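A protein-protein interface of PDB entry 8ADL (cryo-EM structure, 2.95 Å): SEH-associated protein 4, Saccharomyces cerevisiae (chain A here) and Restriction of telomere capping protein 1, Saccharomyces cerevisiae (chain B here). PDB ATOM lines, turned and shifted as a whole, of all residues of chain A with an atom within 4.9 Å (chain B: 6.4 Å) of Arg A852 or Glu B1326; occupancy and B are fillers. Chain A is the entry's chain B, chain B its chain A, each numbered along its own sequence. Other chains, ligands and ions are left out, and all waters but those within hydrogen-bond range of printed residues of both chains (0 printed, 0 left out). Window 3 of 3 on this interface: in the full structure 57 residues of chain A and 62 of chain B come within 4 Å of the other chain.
OG of Ser A848 is in hydrogen-bond range of OE1 of Glu B1326 (3.4 Å). The guanidinium group of Arg A852 lies within salt-bridge range of the side-chain carboxylate of Glu B1326 (2.8 Å). The side-chain carboxylate of Glu B1328 lies within salt-bridge range of the guanidinium group of Arg A852, at 3.2 Å.
The backbone carbonyl oxygen of Glu B1321 lies within hydrogen-bond range of the backbone NH of Glu B1326 (2.9 Å). The backbone carbonyl oxygen of Trp B1322 sits at hydrogen-bond distance from the backbone NH of Glu B1328 (3.3 Å). The side-chain carboxylate (OD2) of Asp A854 lies within salt-bridge range of the guanidinium group (NH1) of Arg A850 (2.9 Å). The side-chain hydroxyl (OG) of Ser A848 is in hydrogen-bond range of the guanidinium group (NH1) of Arg A852, 2.8 Å away.
Ser A848 touches Trp B1322. Pro B1332 touches Arg A850 (O to NH1, 3.8 Å). Trp B1322 touches Ala A851. Ala A851 touches Pro B1332. Arg A852 touches Trp B1322. O of Pro B1332 touches CB of Asp A854 (3.7 Å).
Of chain B, only Trp B1322, Glu B1326 and Glu B1328 come within 4 Å of Arg A852. Of the printed residues of chain B, Ser A848 touches Trp B1322 and Glu B1326. Of the printed residues of chain B, Arg A850 touches Pro B1332. Printed residues of chain A within 4 Å of Trp B1322: Ser A848, Ala A851 and Arg A852. Asp B1325 touches none of the printed residues of chain A. The nearest residue of chain B that does not touch Arg A852 is Pro B1332 (5.5 Å).
Printed residues of chain B that touch a printed residue of chain A: Trp B1322, Glu B1326, Glu B1328 and Pro B1332. Along chain B the printed residues that touch a printed residue of chain A span positions 1322 to 1332. Hydrophobic or aromatic side chains of chain A that line the printed part of chain B: Ala A851. Among the printed residues, Asp or Glu carboxylates within 4 Å of a Lys or Arg side-chain nitrogen of the other chain: Arg A852 with Glu B1326 (2.8 Å) and Arg A852 with Glu B1328 (3.2 Å).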
ATOM      1  N   LEU A 521     -15.648   3.380   9.156  1.00  0.00           N
ATOM      2  CA  LEU A 521     -16.850   4.046   9.644  1.00  0.00           C
ATOM      3  C   LEU A 521     -17.358   5.087   8.655  1.00  0.00           C
ATOM      4  O   LEU A 521     -18.563   5.358   8.607  1.00  0.00           O
ATOM      5  CB  LEU A 521     -16.577   4.683  11.006  1.00  0.00           C
ATOM      6  CG  LEU A 521     -15.860   3.788  12.020  1.00  0.00           C
ATOM      7  CD1 LEU A 521     -15.550   4.556  13.293  1.00  0.00           C
ATOM      8  CD2 LEU A 521     -16.686   2.551  12.327  1.00  0.00           C
ATOM      9  N   SER A 848     -15.537   1.149  22.082  1.00  0.00           N
ATOM     10  CA  SER A 848     -16.180   2.287  21.432  1.00  0.00           C
ATOM     11  C   SER A 848     -16.234   2.104  19.920  1.00  0.00           C
ATOM     12  O   SER A 848     -17.244   2.431  19.282  1.00  0.00           O
ATOM     13  CB  SER A 848     -15.447   3.578  21.794  1.00  0.00           C
ATOM     14  OG  SER A 848     -16.156   4.714  21.330  1.00  0.00           O
ATOM     15  N   MET A 849     -15.166   1.560  19.333  1.00  0.00           N
ATOM     16  CA  MET A 849     -15.172   1.284  17.902  1.00  0.00           C
ATOM     17  C   MET A 849     -16.122   0.145  17.557  1.00  0.00           C
ATOM     18  O   MET A 849     -16.736   0.158  16.485  1.00  0.00           O
ATOM     19  CB  MET A 849     -13.757   0.961  17.426  1.00  0.00           C
ATOM     20  CG  MET A 849     -12.779   2.111  17.580  1.00  0.00           C
ATOM     21  SD  MET A 849     -12.899   3.329  16.262  1.00  0.00           S
ATOM     22  CE  MET A 849     -11.863   4.633  16.919  1.00  0.00           C
ATOM     23  N   ARG A 850     -16.271  -0.833  18.456  1.00  0.00           N
ATOM     24  CA  ARG A 850     -17.255  -1.893  18.253  1.00  0.00           C
ATOM     25  C   ARG A 850     -18.673  -1.335  18.276  1.00  0.00           C
ATOM     26  O   ARG A 850     -19.524  -1.743  17.476  1.00  0.00           O
ATOM     27  CB  ARG A 850     -17.078  -2.974  19.323  1.00  0.00           C
ATOM     28  CG  ARG A 850     -17.713  -4.324  19.007  1.00  0.00           C
ATOM     29  CD  ARG A 850     -19.118  -4.452  19.579  1.00  0.00           C
ATOM     30  NE  ARG A 850     -19.142  -4.284  21.027  1.00  0.00           N
ATOM     31  CZ  ARG A 850     -20.216  -3.928  21.717  1.00  0.00           C
ATOM     32  NH1 ARG A 850     -21.363  -3.653  21.120  1.00  0.00           N
ATOM     33  NH2 ARG A 850     -20.134  -3.834  23.040  1.00  0.00           N
ATOM     34  N   ALA A 851     -18.945  -0.400  19.188  1.00  0.00           N
ATOM     35  CA  ALA A 851     -20.262   0.227  19.239  1.00  0.00           C
ATOM     36  C   ALA A 851     -20.520   1.089  18.006  1.00  0.00           C
ATOM     37  O   ALA A 851     -21.647   1.131  17.496  1.00  0.00           O
ATOM     38  CB  ALA A 851     -20.397   1.046  20.518  1.00  0.00           C
ATOM     39  N   ARG A 852     -19.488   1.789  17.519  1.00  0.00           N
ATOM     40  CA  ARG A 852     -19.623   2.546  16.276  1.00  0.00           C
ATOM     41  C   ARG A 852     -19.887   1.618  15.095  1.00  0.00           C
ATOM     42  O   ARG A 852     -20.683   1.943  14.204  1.00  0.00           O
ATOM     43  CB  ARG A 852     -18.371   3.386  16.028  1.00  0.00           C
ATOM     44  CG  ARG A 852     -18.260   4.615  16.912  1.00  0.00           C
ATOM     45  CD  ARG A 852     -16.882   5.244  16.808  1.00  0.00           C
ATOM     46  NE  ARG A 852     -16.779   6.464  17.599  1.00  0.00           N
ATOM     47  CZ  ARG A 852     -15.908   6.649  18.580  1.00  0.00           C
ATOM     48  NH1 ARG A 852     -15.039   5.711  18.919  1.00  0.00           N
ATOM     49  NH2 ARG A 852     -15.906   7.805  19.237  1.00  0.00           N
ATOM     50  N   PHE A 853     -19.238   0.453  15.083  1.00  0.00           N
ATOM     51  CA  PHE A 853     -19.505  -0.554  14.059  1.00  0.00           C
ATOM     52  C   PHE A 853     -20.944  -1.050  14.134  1.00  0.00           C
ATOM     53  O   PHE A 853     -21.595  -1.243  13.101  1.00  0.00           O
ATOM     54  CB  PHE A 853     -18.523  -1.714  14.218  1.00  0.00           C
ATOM     55  CG  PHE A 853     -18.621  -2.749  13.138  1.00  0.00           C
ATOM     56  CD1 PHE A 853     -18.615  -2.383  11.804  1.00  0.00           C
ATOM     57  CD2 PHE A 853     -18.711  -4.093  13.461  1.00  0.00           C
ATOM     58  CE1 PHE A 853     -18.702  -3.338  10.810  1.00  0.00           C
ATOM     59  CE2 PHE A 853     -18.797  -5.052  12.473  1.00  0.00           C
ATOM     60  CZ  PHE A 853     -18.793  -4.675  11.146  1.00  0.00           C
ATOM     61  N   ASP A 854     -21.458  -1.251  15.350  1.00  0.00           N
ATOM     62  CA  ASP A 854     -22.836  -1.713  15.516  1.00  0.00           C
ATOM     63  C   ASP A 854     -23.845  -0.669  15.043  1.00  0.00           C
ATOM     64  O   ASP A 854     -24.828  -1.011  14.369  1.00  0.00           O
ATOM     65  CB  ASP A 854     -23.092  -2.083  16.976  1.00  0.00           C
ATOM     66  CG  ASP A 854     -22.375  -3.354  17.386  1.00  0.00           C
ATOM     67  OD1 ASP A 854     -21.615  -3.901  16.561  1.00  0.00           O
ATOM     68  OD2 ASP A 854     -22.574  -3.806  18.533  1.00  0.00           O
ATOM     69  N   VAL A 855     -23.625   0.606  15.377  1.00  0.00           N
ATOM     70  CA  VAL A 855     -24.565   1.633  14.924  1.00  0.00           C
ATOM     71  C   VAL A 855     -24.430   1.871  13.422  1.00  0.00           C
ATOM     72  O   VAL A 855     -25.403   2.261  12.763  1.00  0.00           O
ATOM     73  CB  VAL A 855     -24.424   2.940  15.735  1.00  0.00           C
ATOM     74  CG1 VAL A 855     -24.507   2.655  17.217  1.00  0.00           C
ATOM     75  CG2 VAL A 855     -23.140   3.680  15.411  1.00  0.00           C
ATOM     76  N   LEU A 856     -23.251   1.611  12.845  1.00  0.00           N
ATOM     77  CA  LEU A 856     -23.113   1.701  11.395  1.00  0.00           C
ATOM     78  C   LEU A 856     -23.835   0.549  10.707  1.00  0.00           C
ATOM     79  O   LEU A 856     -24.400   0.725   9.622  1.00  0.00           O
ATOM     80  CB  LEU A 856     -21.637   1.725  11.008  1.00  0.00           C
ATOM     81  CG  LEU A 856     -21.326   2.233   9.603  1.00  0.00           C
ATOM     82  CD1 LEU A 856     -21.510   3.739   9.536  1.00  0.00           C
ATOM     83  CD2 LEU A 856     -19.915   1.846   9.198  1.00  0.00           C
ATOM     84  N   GLN B1320     -21.003   6.560  30.663  1.00  0.00           N
ATOM     85  CA  GLN B1320     -20.495   7.924  30.764  1.00  0.00           C
ATOM     86  C   GLN B1320     -19.418   8.195  29.721  1.00  0.00           C
ATOM     87  O   GLN B1320     -19.408   9.269  29.109  1.00  0.00           O
ATOM     88  CB  GLN B1320     -19.955   8.179  32.171  1.00  0.00           C
ATOM     89  CG  GLN B1320     -21.001   8.674  33.157  1.00  0.00           C
ATOM     90  CD  GLN B1320     -20.423   8.932  34.531  1.00  0.00           C
ATOM     91  OE1 GLN B1320     -19.844   9.987  34.785  1.00  0.00           O
ATOM     92  NE2 GLN B1320     -20.575   7.966  35.429  1.00  0.00           N
ATOM     93  N   GLU B1321     -18.521   7.230  29.487  1.00  0.00           N
ATOM     94  CA  GLU B1321     -17.500   7.387  28.454  1.00  0.00           C
ATOM     95  C   GLU B1321     -18.129   7.496  27.072  1.00  0.00           C
ATOM     96  O   GLU B1321     -17.787   8.396  26.294  1.00  0.00           O
ATOM     97  CB  GLU B1321     -16.527   6.209  28.505  1.00  0.00           C
ATOM     98  CG  GLU B1321     -15.355   6.389  29.458  1.00  0.00           C
ATOM     99  CD  GLU B1321     -14.497   5.144  29.557  1.00  0.00           C
ATOM    100  OE1 GLU B1321     -14.918   4.091  29.033  1.00  0.00           O
ATOM    101  OE2 GLU B1321     -13.403   5.216  30.156  1.00  0.00           O
ATOM    102  N   TRP B1322     -19.101   6.625  26.780  1.00  0.00           N
ATOM    103  CA  TRP B1322     -19.734   6.601  25.465  1.00  0.00           C
ATOM    104  C   TRP B1322     -20.540   7.868  25.194  1.00  0.00           C
ATOM    105  O   TRP B1322     -20.590   8.339  24.051  1.00  0.00           O
ATOM    106  CB  TRP B1322     -20.612   5.355  25.338  1.00  0.00           C
ATOM    107  CG  TRP B1322     -21.439   5.301  24.092  1.00  0.00           C
ATOM    108  CD1 TRP B1322     -22.779   5.520  23.992  1.00  0.00           C
ATOM    109  CD2 TRP B1322     -20.976   5.031  22.766  1.00  0.00           C
ATOM    110  NE1 TRP B1322     -23.185   5.387  22.687  1.00  0.00           N
ATOM    111  CE2 TRP B1322     -22.095   5.087  21.915  1.00  0.00           C
ATOM    112  CE3 TRP B1322     -19.725   4.738  22.217  1.00  0.00           C
ATOM    113  CZ2 TRP B1322     -22.002   4.866  20.545  1.00  0.00           C
ATOM    114  CZ3 TRP B1322     -19.633   4.522  20.859  1.00  0.00           C
ATOM    115  CH2 TRP B1322     -20.764   4.587  20.036  1.00  0.00           C
ATOM    116  N   PHE B1323     -21.171   8.445  26.216  1.00  0.00           N
ATOM    117  CA  PHE B1323     -22.045   9.586  25.976  1.00  0.00           C
ATOM    118  C   PHE B1323     -21.419  10.940  26.302  1.00  0.00           C
ATOM    119  O   PHE B1323     -22.028  11.966  25.982  1.00  0.00           O
ATOM    120  CB  PHE B1323     -23.356   9.422  26.753  1.00  0.00           C
ATOM    121  CG  PHE B1323     -24.291   8.412  26.151  1.00  0.00           C
ATOM    122  CD1 PHE B1323     -24.761   8.569  24.857  1.00  0.00           C
ATOM    123  CD2 PHE B1323     -24.694   7.303  26.871  1.00  0.00           C
ATOM    124  CE1 PHE B1323     -25.622   7.642  24.301  1.00  0.00           C
ATOM    125  CE2 PHE B1323     -25.553   6.373  26.319  1.00  0.00           C
ATOM    126  CZ  PHE B1323     -26.018   6.544  25.033  1.00  0.00           C
ATOM    127  N   LEU B1324     -20.240  10.983  26.925  1.00  0.00           N
ATOM    128  CA  LEU B1324     -19.550  12.245  27.166  1.00  0.00           C
ATOM    129  C   LEU B1324     -18.170  12.297  26.527  1.00  0.00           C
ATOM    130  O   LEU B1324     -17.844  13.278  25.847  1.00  0.00           O
ATOM    131  CB  LEU B1324     -19.429  12.514  28.677  1.00  0.00           C
ATOM    132  CG  LEU B1324     -20.598  12.314  29.640  1.00  0.00           C
ATOM    133  CD1 LEU B1324     -20.098  12.520  31.061  1.00  0.00           C
ATOM    134  CD2 LEU B1324     -21.719  13.282  29.316  1.00  0.00           C
ATOM    135  N   ASP B1325     -17.344  11.266  26.727  1.00  0.00           N
ATOM    136  CA  ASP B1325     -15.975  11.316  26.227  1.00  0.00           C
ATOM    137  C   ASP B1325     -15.931  11.110  24.719  1.00  0.00           C
ATOM    138  O   ASP B1325     -15.175  11.790  24.014  1.00  0.00           O
ATOM    139  CB  ASP B1325     -15.125  10.272  26.948  1.00  0.00           C
ATOM    140  CG  ASP B1325     -15.194  10.412  28.460  1.00  0.00           C
ATOM    141  OD1 ASP B1325     -15.850  11.357  28.948  1.00  0.00           O
ATOM    142  OD2 ASP B1325     -14.568   9.593  29.162  1.00  0.00           O
ATOM    143  N   GLU B1326     -16.738  10.189  24.203  1.00  0.00           N
ATOM    144  CA  GLU B1326     -16.805   9.974  22.768  1.00  0.00           C
ATOM    145  C   GLU B1326     -17.831  10.868  22.087  1.00  0.00           C
ATOM    146  O   GLU B1326     -17.845  10.924  20.852  1.00  0.00           O
ATOM    147  CB  GLU B1326     -17.121   8.506  22.473  1.00  0.00           C
ATOM    148  CG  GLU B1326     -16.290   7.529  23.284  1.00  0.00           C
ATOM    149  CD  GLU B1326     -14.824   7.554  22.906  1.00  0.00           C
ATOM    150  OE1 GLU B1326     -14.517   7.699  21.705  1.00  0.00           O
ATOM    151  OE2 GLU B1326     -13.976   7.425  23.816  1.00  0.00           O
ATOM    152  N   ASN B1327     -18.660  11.573  22.869  1.00  0.00           N
ATOM    153  CA  ASN B1327     -19.676  12.514  22.377  1.00  0.00           C
ATOM    154  C   ASN B1327     -20.626  11.857  21.379  1.00  0.00           C
ATOM    155  O   ASN B1327     -20.980  12.440  20.352  1.00  0.00           O
ATOM    156  CB  ASN B1327     -19.035  13.768  21.776  1.00  0.00           C
ATOM    157  CG  ASN B1327     -19.084  14.955  22.717  1.00  0.00           C
ATOM    158  OD1 ASN B1327     -20.095  15.196  23.378  1.00  0.00           O
ATOM    159  ND2 ASN B1327     -17.991  15.707  22.782  1.00  0.00           N
ATOM    160  N   GLU B1328     -21.044  10.637  21.685  1.00  0.00           N
ATOM    161  CA  GLU B1328     -21.949   9.880  20.837  1.00  0.00           C
ATOM    162  C   GLU B1328     -23.390  10.057  21.300  1.00  0.00           C
ATOM    163  O   GLU B1328     -23.659  10.462  22.434  1.00  0.00           O
ATOM    164  CB  GLU B1328     -21.570   8.400  20.839  1.00  0.00           C
ATOM    165  CG  GLU B1328     -20.188   8.122  20.273  1.00  0.00           C
ATOM    166  CD  GLU B1328     -20.135   8.250  18.765  1.00  0.00           C
ATOM    167  OE1 GLU B1328     -21.157   7.968  18.105  1.00  0.00           O
ATOM    168  OE2 GLU B1328     -19.071   8.634  18.238  1.00  0.00           O
ATOM    169  N   PRO B1332     -24.984   1.996  22.357  1.00  0.00           N
ATOM    170  CA  PRO B1332     -23.852   1.167  21.909  1.00  0.00           C
ATOM    171  C   PRO B1332     -24.257  -0.118  21.207  1.00  0.00           C
ATOM    172  O   PRO B1332     -23.518  -0.596  20.338  1.00  0.00           O
ATOM    173  CB  PRO B1332     -23.100   0.881  23.214  1.00  0.00           C
ATOM    174  CG  PRO B1332     -23.414   2.046  24.076  1.00  0.00           C
ATOM    175  CD  PRO B1332     -24.838   2.409  23.764  1.00  0.00           C
